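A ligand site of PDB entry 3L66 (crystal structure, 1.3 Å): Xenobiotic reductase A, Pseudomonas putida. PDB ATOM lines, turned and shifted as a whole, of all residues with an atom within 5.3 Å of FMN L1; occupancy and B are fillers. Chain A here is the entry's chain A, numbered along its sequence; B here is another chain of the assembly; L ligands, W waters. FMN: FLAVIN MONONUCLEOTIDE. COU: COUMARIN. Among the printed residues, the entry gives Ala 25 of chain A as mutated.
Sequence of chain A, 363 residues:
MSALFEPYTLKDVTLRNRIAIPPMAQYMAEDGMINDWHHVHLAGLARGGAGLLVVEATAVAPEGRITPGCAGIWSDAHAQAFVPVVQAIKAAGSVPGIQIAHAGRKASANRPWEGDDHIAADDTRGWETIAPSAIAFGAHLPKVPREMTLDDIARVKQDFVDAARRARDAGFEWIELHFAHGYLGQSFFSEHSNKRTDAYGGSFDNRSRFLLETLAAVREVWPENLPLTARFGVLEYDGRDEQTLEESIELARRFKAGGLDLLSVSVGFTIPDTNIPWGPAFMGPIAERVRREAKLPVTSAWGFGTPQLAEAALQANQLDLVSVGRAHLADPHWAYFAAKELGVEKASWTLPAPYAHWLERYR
O3P of FMN L1 is in hydrogen-bond range of N of Gly 325, at 2.8 Å. The backbone NH (N) of Arg 326 sits at hydrogen-bond distance from an oxygen (O1P) of FMN L1 (2.8 Å). O1P of FMN L1 lies within salt-bridge range of NE of Arg 326, 2.8 Å away. The backbone NH of Ala 25 sits at hydrogen-bond distance from a nitrogen (N5) of FMN L1. The backbone NH (N) of Gly 303 is in hydrogen-bond range of an oxygen (O2P) of FMN L1 (2.9 Å). An oxygen (O2) of FMN L1 sits at hydrogen-bond distance from the guanidinium group (NH2) of Arg 231, 2.9 Å away. The side-chain amide oxygen (OE1) of Gln 99 lies within hydrogen-bond range of a nitrogen (N3) of FMN L1 (2.9 Å). The backbone carbonyl oxygen of Pro 23 lies within hydrogen-bond range of an oxygen (O2') of FMN L1 (2.9 Å). N of Ala 57 sits at hydrogen-bond distance from O4 of FMN L1 (3.0 Å). The backbone NH (N) of Trp 302 is in hydrogen-bond range of an oxygen (O5') of FMN L1 (3.4 Å). A ring nitrogen (NE2) of His 178 is in hydrogen-bond range of an oxygen (O2) of FMN L1 (3.2 Å). O2 of FMN L1 lies close to ND1 of His 181, 3.5 Å away. A ring nitrogen (NE2) of His 178 is in hydrogen-bond range of an oxygen (O1) of COU L2, at 2.9 Å. ND1 of His 181 sits at hydrogen-bond distance from O1 of COU L2 (2.9 Å).
Water W2 lies within hydrogen-bond range of an oxygen (O3P) of FMN L1 (2.8 Å), the backbone NH (N) of Ala 327 (2.8 Å) and the backbone NH (N) of Arg 326 (3.4 Å). Water W1 lies within hydrogen-bond range of an oxygen (O2P) of FMN L1 (2.8 Å) and the guanidinium group of Arg 326 (3.3 Å).
A nitrogen (N3) of FMN L1 sits close to an oxygen (O1) of COU L2 (3.2 Å).
Residues that only touch FMN L1: Pro 22, Met 24, Glu 56, Ala 301, Val 324, Leu 329 and Trp 358 of chain B. Hydrophobic or aromatic side chains within 4 Å of FMN L1: Pro 22, Pro 23, Met 24, Ala 25, Ala 57, His 178, His 181, Ala 301, Trp 302, Leu 329 and Trp 358 of chain B. Within 4 Å of FMN L1: Pro 22, Pro 23, Met 24, Ala 25, Glu 56, Ala 57, Gln 99, His 178, His 181, Arg 231, Ala 301, Trp 302, Gly 303, Val 324, Gly 325, Arg 326, Leu 329 and Trp 358 of chain B. The nearest printed residue that does not touch FMN L1 is Ser 323 (4.2 Å).
OE1 of Gln 99 lies close to N of Ala 57, 3.4 Å away. The side-chain amide nitrogen (NE2) of Gln 99 lies within hydrogen-bond range of the side-chain carboxylate (OE2) of Glu 176. The indole nitrogen (NE1) of Trp 358 of chain B lies close to the backbone carbonyl oxygen (O) of Pro 354 of chain B (3.4 Å). O of Met 24 sits at hydrogen-bond distance from NE2 of Gln 26 (3.0 Å). N of Gln 26 is in hydrogen-bond range of OE1 of Glu 56 (3.0 Å).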
ATOM      1  N   PRO A  22     -26.880  11.023  20.644  1.00  0.00           N
ATOM      2  CA  PRO A  22     -25.631  10.363  21.035  1.00  0.00           C
ATOM      3  C   PRO A  22     -25.170   9.479  19.880  1.00  0.00           C
ATOM      4  O   PRO A  22     -25.970   9.158  18.988  1.00  0.00           O
ATOM      5  CB  PRO A  22     -26.045   9.493  22.232  1.00  0.00           C
ATOM      6  CG  PRO A  22     -27.509   9.171  21.953  1.00  0.00           C
ATOM      7  CD  PRO A  22     -28.058  10.417  21.287  1.00  0.00           C
ATOM      8  N   PRO A  23     -23.914   9.049  19.910  1.00  0.00           N
ATOM      9  CA  PRO A  23     -23.426   8.145  18.884  1.00  0.00           C
ATOM     10  C   PRO A  23     -24.259   6.866  18.806  1.00  0.00           C
ATOM     11  O   PRO A  23     -24.535   6.214  19.826  1.00  0.00           O
ATOM     12  CB  PRO A  23     -21.993   7.840  19.344  1.00  0.00           C
ATOM     13  CG  PRO A  23     -22.022   8.075  20.851  1.00  0.00           C
ATOM     14  CD  PRO A  23     -22.927   9.276  20.990  1.00  0.00           C
ATOM     15  N   MET A  24     -24.660   6.514  17.587  1.00  0.00           N
ATOM     16  CA  MET A  24     -25.409   5.283  17.356  1.00  0.00           C
ATOM     17  C   MET A  24     -24.863   4.572  16.108  1.00  0.00           C
ATOM     18  O   MET A  24     -25.190   4.952  14.962  1.00  0.00           O
ATOM     19  CB  MET A  24     -26.908   5.559  17.220  1.00  0.00           C
ATOM     20  CG  MET A  24     -27.565   5.863  18.575  1.00  0.00           C
ATOM     21  SD  MET A  24     -29.366   6.150  18.382  1.00  0.00           S
ATOM     22  CE  MET A  24     -29.341   7.713  17.549  1.00  0.00           C
ATOM     23  N   ALA A  25     -24.080   3.539  16.361  1.00  0.00           N
ATOM     24  CA  ALA A  25     -23.550   2.641  15.337  1.00  0.00           C
ATOM     25  C   ALA A  25     -24.643   2.199  14.364  1.00  0.00           C
ATOM     26  O   ALA A  25     -25.728   1.792  14.779  1.00  0.00           O
ATOM     27  CB  ALA A  25     -22.923   1.448  15.991  1.00  0.00           C
ATOM     28  N   GLN A  26     -24.325   2.302  13.080  1.00  0.00           N
ATOM     29  CA  GLN A  26     -25.234   1.946  12.007  1.00  0.00           C
ATOM     30  C   GLN A  26     -24.906   0.603  11.313  1.00  0.00           C
ATOM     31  O   GLN A  26     -25.760   0.028  10.625  1.00  0.00           O
ATOM     32  CB  GLN A  26     -25.288   3.063  10.971  1.00  0.00           C
ATOM     33  CG  GLN A  26     -25.849   4.373  11.528  1.00  0.00           C
ATOM     34  CD  GLN A  26     -27.280   4.246  11.960  1.00  0.00           C
ATOM     35  OE1 GLN A  26     -28.175   4.154  11.099  1.00  0.00           O
ATOM     36  NE2 GLN A  26     -27.519   4.188  13.260  1.00  0.00           N
ATOM     37  N   TYR A  27     -23.665   0.154  11.442  1.00  0.00           N
ATOM     38  CA  TYR A  27     -23.237  -1.136  10.907  1.00  0.00           C
ATOM     39  C   TYR A  27     -23.420  -1.203   9.385  1.00  0.00           C
ATOM     40  O   TYR A  27     -23.671  -2.276   8.840  1.00  0.00           O
ATOM     41  CB  TYR A  27     -23.919  -2.310  11.612  1.00  0.00           C
ATOM     42  CG  TYR A  27     -23.868  -2.224  13.128  1.00  0.00           C
ATOM     43  CD1 TYR A  27     -22.778  -2.735  13.825  1.00  0.00           C
ATOM     44  CD2 TYR A  27     -24.856  -1.561  13.847  1.00  0.00           C
ATOM     45  CE1 TYR A  27     -22.708  -2.641  15.214  1.00  0.00           C
ATOM     46  CE2 TYR A  27     -24.787  -1.467  15.235  1.00  0.00           C
ATOM     47  CZ  TYR A  27     -23.732  -2.015  15.904  1.00  0.00           C
ATOM     48  OH  TYR A  27     -23.702  -1.897  17.283  1.00  0.00           O
ATOM     49  N   GLU A  56     -21.640   8.113  15.237  1.00  0.00           N
ATOM     50  CA  GLU A  56     -21.362   6.800  15.779  1.00  0.00           C
ATOM     51  C   GLU A  56     -19.892   6.503  16.028  1.00  0.00           C
ATOM     52  O   GLU A  56     -18.995   7.075  15.387  1.00  0.00           O
ATOM     53  CB  GLU A  56     -21.890   5.738  14.803  1.00  0.00           C
ATOM     54  CG  GLU A  56     -21.133   5.704  13.458  1.00  0.00           C
ATOM     55  CD  GLU A  56     -21.936   4.941  12.431  1.00  0.00           C
ATOM     56  OE1 GLU A  56     -21.803   3.722  12.341  1.00  0.00           O
ATOM     57  OE2 GLU A  56     -22.726   5.558  11.688  1.00  0.00           O
ATOM     58  N   ALA A  57     -19.684   5.537  16.924  1.00  0.00           N
ATOM     59  CA  ALA A  57     -18.340   4.988  17.196  1.00  0.00           C
ATOM     60  C   ALA A  57     -17.576   4.764  15.893  1.00  0.00           C
ATOM     61  O   ALA A  57     -17.941   3.887  15.117  1.00  0.00           O
ATOM     62  CB  ALA A  57     -18.435   3.697  18.003  1.00  0.00           C
ATOM     63  N   GLN A  99     -17.651  10.445  17.726  1.00  0.00           N
ATOM     64  CA  GLN A  99     -17.072   9.592  18.757  1.00  0.00           C
ATOM     65  C   GLN A  99     -15.990   8.724  18.112  1.00  0.00           C
ATOM     66  O   GLN A  99     -16.282   7.965  17.194  1.00  0.00           O
ATOM     67  CB  GLN A  99     -18.164   8.716  19.398  1.00  0.00           C
ATOM     68  CG  GLN A  99     -17.622   7.883  20.540  1.00  0.00           C
ATOM     69  CD  GLN A  99     -18.624   6.852  21.006  1.00  0.00           C
ATOM     70  OE1 GLN A  99     -19.008   5.952  20.237  1.00  0.00           O
ATOM     71  NE2 GLN A  99     -19.005   6.922  22.289  1.00  0.00           N
ATOM     72  N   GLU A 176     -15.615  13.156  20.947  1.00  0.00           N
ATOM     73  CA  GLU A 176     -15.902  12.313  22.078  1.00  0.00           C
ATOM     74  C   GLU A 176     -15.011  11.084  22.038  1.00  0.00           C
ATOM     75  O   GLU A 176     -15.086  10.268  21.124  1.00  0.00           O
ATOM     76  CB  GLU A 176     -17.388  11.910  22.120  1.00  0.00           C
ATOM     77  CG  GLU A 176     -17.793  11.154  23.356  1.00  0.00           C
ATOM     78  CD  GLU A 176     -19.238  10.693  23.330  1.00  0.00           C
ATOM     79  OE1 GLU A 176     -20.134  11.511  23.490  1.00  0.00           O
ATOM     80  OE2 GLU A 176     -19.480   9.505  23.164  1.00  0.00           O
ATOM     81  N   HIS A 178     -14.211   7.463  23.136  1.00  0.00           N
ATOM     82  CA  HIS A 178     -15.044   6.349  23.627  1.00  0.00           C
ATOM     83  C   HIS A 178     -14.315   5.499  24.644  1.00  0.00           C
ATOM     84  O   HIS A 178     -13.663   4.504  24.301  1.00  0.00           O
ATOM     85  CB  HIS A 178     -15.493   5.464  22.479  1.00  0.00           C
ATOM     86  CG  HIS A 178     -16.662   4.615  22.804  1.00  0.00           C
ATOM     87  ND1 HIS A 178     -17.149   4.496  24.080  1.00  0.00           N
ATOM     88  CD2 HIS A 178     -17.491   3.907  22.007  1.00  0.00           C
ATOM     89  CE1 HIS A 178     -18.231   3.738  24.053  1.00  0.00           C
ATOM     90  NE2 HIS A 178     -18.474   3.388  22.799  1.00  0.00           N
ATOM     91  N   HIS A 181     -18.424   1.370  27.821  1.00  0.00           N
ATOM     92  CA  HIS A 181     -19.128   0.233  27.206  1.00  0.00           C
ATOM     93  C   HIS A 181     -18.272  -0.998  26.994  1.00  0.00           C
ATOM     94  O   HIS A 181     -18.600  -1.871  26.170  1.00  0.00           O
ATOM     95  CB  HIS A 181     -19.839   0.680  25.920  1.00  0.00           C
ATOM     96  CG  HIS A 181     -20.825   1.771  26.165  1.00  0.00           C
ATOM     97  ND1 HIS A 181     -21.470   2.451  25.144  1.00  0.00           N
ATOM     98  CD2 HIS A 181     -21.321   2.284  27.323  1.00  0.00           C
ATOM     99  CE1 HIS A 181     -22.286   3.346  25.665  1.00  0.00           C
ATOM    100  NE2 HIS A 181     -22.200   3.268  26.975  1.00  0.00           N
ATOM    101  N   ARG A 231     -16.800   9.695  26.692  1.00  0.00           N
ATOM    102  CA  ARG A 231     -17.830   8.847  27.271  1.00  0.00           C
ATOM    103  C   ARG A 231     -17.132   7.825  28.157  1.00  0.00           C
ATOM    104  O   ARG A 231     -16.139   7.226  27.748  1.00  0.00           O
ATOM    105  CB  ARG A 231     -18.690   8.193  26.167  1.00  0.00           C
ATOM    106  CG  ARG A 231     -20.004   7.654  26.717  1.00  0.00           C
ATOM    107  CD  ARG A 231     -20.967   7.198  25.630  1.00  0.00           C
ATOM    108  NE  ARG A 231     -22.327   7.318  26.143  1.00  0.00           N
ATOM    109  CZ  ARG A 231     -23.428   7.088  25.439  1.00  0.00           C
ATOM    110  NH1 ARG A 231     -24.632   7.355  25.962  1.00  0.00           N
ATOM    111  NH2 ARG A 231     -23.363   6.546  24.227  1.00  0.00           N
ATOM    112  N   ALA A 301     -27.889   9.230  29.016  1.00  0.00           N
ATOM    113  CA  ALA A 301     -28.870   8.656  28.102  1.00  0.00           C
ATOM    114  C   ALA A 301     -29.528   7.465  28.801  1.00  0.00           C
ATOM    115  O   ALA A 301     -29.254   7.197  29.935  1.00  0.00           O
ATOM    116  CB  ALA A 301     -28.194   8.216  26.809  1.00  0.00           C
ATOM    117  N   TRP A 302     -30.638   7.045  28.181  1.00  0.00           N
ATOM    118  CA  TRP A 302     -31.455   5.852  28.413  1.00  0.00           C
ATOM    119  C   TRP A 302     -32.852   6.277  28.851  1.00  0.00           C
ATOM    120  O   TRP A 302     -33.090   6.550  30.064  1.00  0.00           O
ATOM    121  CB  TRP A 302     -30.898   4.832  29.399  1.00  0.00           C
ATOM    122  CG  TRP A 302     -31.778   3.600  29.395  1.00  0.00           C
ATOM    123  CD1 TRP A 302     -32.955   3.382  30.104  1.00  0.00           C
ATOM    124  CD2 TRP A 302     -31.573   2.427  28.605  1.00  0.00           C
ATOM    125  NE1 TRP A 302     -33.437   2.151  29.836  1.00  0.00           N
ATOM    126  CE2 TRP A 302     -32.628   1.544  28.901  1.00  0.00           C
ATOM    127  CE3 TRP A 302     -30.561   2.016  27.738  1.00  0.00           C
ATOM    128  CZ2 TRP A 302     -32.733   0.288  28.298  1.00  0.00           C
ATOM    129  CZ3 TRP A 302     -30.674   0.769  27.127  1.00  0.00           C
ATOM    130  CH2 TRP A 302     -31.742  -0.076  27.414  1.00  0.00           C
ATOM    131  N   GLY A 303     -33.788   6.287  27.900  1.00  0.00           N
ATOM    132  CA  GLY A 303     -35.180   6.585  28.165  1.00  0.00           C
ATOM    133  C   GLY A 303     -35.585   8.043  28.214  1.00  0.00           C
ATOM    134  O   GLY A 303     -36.678   8.346  28.699  1.00  0.00           O
ATOM    135  N   PHE A 304     -34.762   8.953  27.715  1.00  0.00           N
ATOM    136  CA  PHE A 304     -35.136  10.363  27.718  1.00  0.00           C
ATOM    137  C   PHE A 304     -35.976  10.792  26.496  1.00  0.00           C
ATOM    138  O   PHE A 304     -36.250  11.979  26.327  1.00  0.00           O
ATOM    139  CB  PHE A 304     -33.920  11.280  27.896  1.00  0.00           C
ATOM    140  CG  PHE A 304     -33.282  11.189  29.253  1.00  0.00           C
ATOM    141  CD1 PHE A 304     -33.831  11.873  30.332  1.00  0.00           C
ATOM    142  CD2 PHE A 304     -32.147  10.433  29.465  1.00  0.00           C
ATOM    143  CE1 PHE A 304     -33.244  11.820  31.565  1.00  0.00           C
ATOM    144  CE2 PHE A 304     -31.539  10.383  30.692  1.00  0.00           C
ATOM    145  CZ  PHE A 304     -32.087  11.076  31.742  1.00  0.00           C
ATOM    146  N   GLY A 305     -36.430   9.840  25.704  1.00  0.00           N
ATOM    147  CA  GLY A 305     -37.340  10.132  24.611  1.00  0.00           C
ATOM    148  C   GLY A 305     -38.717  10.611  25.048  1.00  0.00           C
ATOM    149  O   GLY A 305     -39.498  11.055  24.233  1.00  0.00           O
ATOM    150  N   SER A 323     -29.147  13.328  26.124  1.00  0.00           N
ATOM    151  CA  SER A 323     -28.924  12.508  24.942  1.00  0.00           C
ATOM    152  C   SER A 323     -30.140  11.609  24.707  1.00  0.00           C
ATOM    153  O   SER A 323     -30.542  10.881  25.596  1.00  0.00           O
ATOM    154  CB  SER A 323     -27.660  11.688  25.077  1.00  0.00           C
ATOM    155  OG  SER A 323     -26.513  12.529  25.140  1.00  0.00           O
ATOM    156  N   VAL A 324     -30.635  11.626  23.465  1.00  0.00           N
ATOM    157  CA  VAL A 324     -31.863  10.941  23.053  1.00  0.00           C
ATOM    158  C   VAL A 324     -31.522  10.116  21.805  1.00  0.00           C
ATOM    159  O   VAL A 324     -31.315  10.685  20.714  1.00  0.00           O
ATOM    160  CB  VAL A 324     -33.008  11.947  22.805  1.00  0.00           C
ATOM    161  CG1 VAL A 324     -34.241  11.178  22.317  1.00  0.00           C
ATOM    162  CG2 VAL A 324     -33.307  12.779  24.054  1.00  0.00           C
ATOM    163  N   GLY A 325     -31.422   8.802  21.992  1.00  0.00           N
ATOM    164  CA  GLY A 325     -30.943   7.866  20.967  1.00  0.00           C
ATOM    165  C   GLY A 325     -32.059   7.205  20.177  1.00  0.00           C
ATOM    166  O   GLY A 325     -32.412   7.644  19.070  1.00  0.00           O
ATOM    167  N   ARG A 326     -32.622   6.134  20.715  1.00  0.00           N
ATOM    168  CA  ARG A 326     -33.602   5.334  19.964  1.00  0.00           C
ATOM    169  C   ARG A 326     -34.811   6.128  19.471  1.00  0.00           C
ATOM    170  O   ARG A 326     -35.347   5.870  18.370  1.00  0.00           O
ATOM    171  CB  ARG A 326     -34.017   4.114  20.775  1.00  0.00           C
ATOM    172  CG  ARG A 326     -32.925   3.060  20.767  1.00  0.00           C
ATOM    173  CD  ARG A 326     -33.184   1.984  21.765  1.00  0.00           C
ATOM    174  NE  ARG A 326     -33.058   2.501  23.122  1.00  0.00           N
ATOM    175  CZ  ARG A 326     -33.205   1.748  24.179  1.00  0.00           C
ATOM    176  NH1 ARG A 326     -33.436   0.440  24.025  1.00  0.00           N
ATOM    177  NH2 ARG A 326     -33.106   2.296  25.378  1.00  0.00           N
ATOM    178  N   ALA A 327     -35.276   7.097  20.234  1.00  0.00           N
ATOM    179  CA  ALA A 327     -36.414   7.884  19.788  1.00  0.00           C
ATOM    180  C   ALA A 327     -36.130   8.576  18.441  1.00  0.00           C
ATOM    181  O   ALA A 327     -37.064   8.846  17.673  1.00  0.00           O
ATOM    182  CB  ALA A 327     -36.815   8.906  20.863  1.00  0.00           C
ATOM    183  N   LEU A 329     -34.174   7.231  16.032  1.00  0.00           N
ATOM    184  CA  LEU A 329     -34.275   6.203  14.990  1.00  0.00           C
ATOM    185  C   LEU A 329     -35.750   6.028  14.614  1.00  0.00           C
ATOM    186  O   LEU A 329     -36.101   5.887  13.433  1.00  0.00           O
ATOM    187  CB  LEU A 329     -33.684   4.876  15.484  1.00  0.00           C
ATOM    188  CG  LEU A 329     -32.257   4.939  16.059  1.00  0.00           C
ATOM    189  CD1 LEU A 329     -31.790   3.559  16.457  1.00  0.00           C
ATOM    190  CD2 LEU A 329     -31.283   5.580  15.037  1.00  0.00           C
ATOM    191  N   PRO B 354     -30.858  -1.064  10.396  1.00  0.00           N
ATOM    192  CA  PRO B 354     -30.161  -0.268  11.418  1.00  0.00           C
ATOM    193  C   PRO B 354     -31.086   0.534  12.327  1.00  0.00           C
ATOM    194  O   PRO B 354     -30.596   1.064  13.339  1.00  0.00           O
ATOM    195  CB  PRO B 354     -29.282   0.690  10.601  1.00  0.00           C
ATOM    196  CG  PRO B 354     -29.151   0.000   9.247  1.00  0.00           C
ATOM    197  CD  PRO B 354     -30.433  -0.716   9.025  1.00  0.00           C
ATOM    198  N   TRP B 358     -33.587  -2.246  16.650  1.00  0.00           N
ATOM    199  CA  TRP B 358     -33.538  -1.641  17.979  1.00  0.00           C
ATOM    200  C   TRP B 358     -34.892  -1.195  18.496  1.00  0.00           C
ATOM    201  O   TRP B 358     -35.013  -0.785  19.647  1.00  0.00           O
ATOM    202  CB  TRP B 358     -32.629  -0.396  17.913  1.00  0.00           C
ATOM    203  CG  TRP B 358     -31.332  -0.742  17.333  1.00  0.00           C
ATOM    204  CD1 TRP B 358     -30.881  -0.405  16.090  1.00  0.00           C
ATOM    205  CD2 TRP B 358     -30.331  -1.565  17.923  1.00  0.00           C
ATOM    206  NE1 TRP B 358     -29.657  -0.971  15.861  1.00  0.00           N
ATOM    207  CE2 TRP B 358     -29.284  -1.680  16.984  1.00  0.00           C
ATOM    208  CE3 TRP B 358     -30.206  -2.228  19.153  1.00  0.00           C
ATOM    209  CZ2 TRP B 358     -28.118  -2.368  17.252  1.00  0.00           C
ATOM    210  CZ3 TRP B 358     -29.042  -2.947  19.400  1.00  0.00           C
ATOM    211  CH2 TRP B 358     -28.018  -3.006  18.445  1.00  0.00           C
HETATM  212  N1  FMN L   1     -23.164   4.206  22.361  1.00  0.00           N
HETATM  213  C2  FMN L   1     -21.910   4.627  22.145  1.00  0.00           C
HETATM  214  O2  FMN L   1     -21.184   5.158  22.970  1.00  0.00           O
HETATM  215  N3  FMN L   1     -21.442   4.518  20.803  1.00  0.00           N
HETATM  216  C4  FMN L   1     -22.132   3.986  19.796  1.00  0.00           C
HETATM  217  O4  FMN L   1     -21.673   4.033  18.598  1.00  0.00           O
HETATM  218  C4A FMN L   1     -23.363   3.391  20.131  1.00  0.00           C
HETATM  219  N5  FMN L   1     -24.104   2.829  19.094  1.00  0.00           N
HETATM  220  C5A FMN L   1     -25.434   2.542  19.408  1.00  0.00           C
HETATM  221  C6  FMN L   1     -26.189   2.028  18.347  1.00  0.00           C
HETATM  222  C7  FMN L   1     -27.596   1.883  18.463  1.00  0.00           C
HETATM  223  C7M FMN L   1     -28.499   1.564  17.282  1.00  0.00           C
HETATM  224  C8  FMN L   1     -28.170   2.135  19.724  1.00  0.00           C
HETATM  225  C8M FMN L   1     -29.659   1.980  19.927  1.00  0.00           C
HETATM  226  C9  FMN L   1     -27.372   2.555  20.804  1.00  0.00           C
HETATM  227  C9A FMN L   1     -25.970   2.798  20.622  1.00  0.00           C
HETATM  228  N10 FMN L   1     -25.202   3.332  21.640  1.00  0.00           N
HETATM  229  C10 FMN L   1     -23.900   3.648  21.373  1.00  0.00           C
HETATM  230  C1' FMN L   1     -25.843   3.827  22.919  1.00  0.00           C
HETATM  231  C2' FMN L   1     -26.637   5.052  22.695  1.00  0.00           C
HETATM  232  O2' FMN L   1     -25.737   6.176  22.455  1.00  0.00           O
HETATM  233  C3' FMN L   1     -27.496   5.449  23.903  1.00  0.00           C
HETATM  234  O3' FMN L   1     -26.696   5.559  25.077  1.00  0.00           O
HETATM  235  C4' FMN L   1     -28.598   4.416  24.187  1.00  0.00           C
HETATM  236  O4' FMN L   1     -29.313   4.096  22.973  1.00  0.00           O
HETATM  237  C5' FMN L   1     -29.507   4.883  25.277  1.00  0.00           C
HETATM  238  O5' FMN L   1     -30.267   6.058  24.950  1.00  0.00           O
HETATM  239  P   FMN L   1     -31.824   5.895  24.428  1.00  0.00           P
HETATM  240  O1P FMN L   1     -31.789   5.012  23.197  1.00  0.00           O
HETATM  241  O2P FMN L   1     -32.631   5.182  25.517  1.00  0.00           O
HETATM  242  O3P FMN L   1     -32.216   7.262  24.184  1.00  0.00           O
HETATM  243  C1  COU L   2     -21.801   1.178  21.824  1.00  0.00           C
HETATM  244  C2  COU L   2     -21.720   0.754  20.481  1.00  0.00           C
HETATM  245  C3  COU L   2     -22.805   0.116  19.876  1.00  0.00           C
HETATM  246  C4  COU L   2     -23.961  -0.117  20.650  1.00  0.00           C
HETATM  247  C5  COU L   2     -25.117  -0.734  20.133  1.00  0.00           C
HETATM  248  C6  COU L   2     -26.202  -0.934  20.945  1.00  0.00           C
HETATM  249  C7  COU L   2     -26.198  -0.497  22.278  1.00  0.00           C
HETATM  250  C8  COU L   2     -25.076   0.104  22.801  1.00  0.00           C
HETATM  251  C9  COU L   2     -23.984   0.305  21.982  1.00  0.00           C
HETATM  252  O1  COU L   2     -20.915   1.805  22.406  1.00  0.00           O
HETATM  253  O2  COU L   2     -22.918   0.930  22.565  1.00  0.00           O
HETATM  254  O   HOH W   1     -35.361   4.657  25.114  1.00  0.00           O
HETATM  255  O   HOH W   2     -34.705   7.605  22.958  1.00  0.00           O
HETATM  256  O   HOH W   3     -29.643   1.218  23.762  1.00  0.00           O
HETATM  257  O   HOH W   4     -32.105   8.722  26.417  1.00  0.00           O
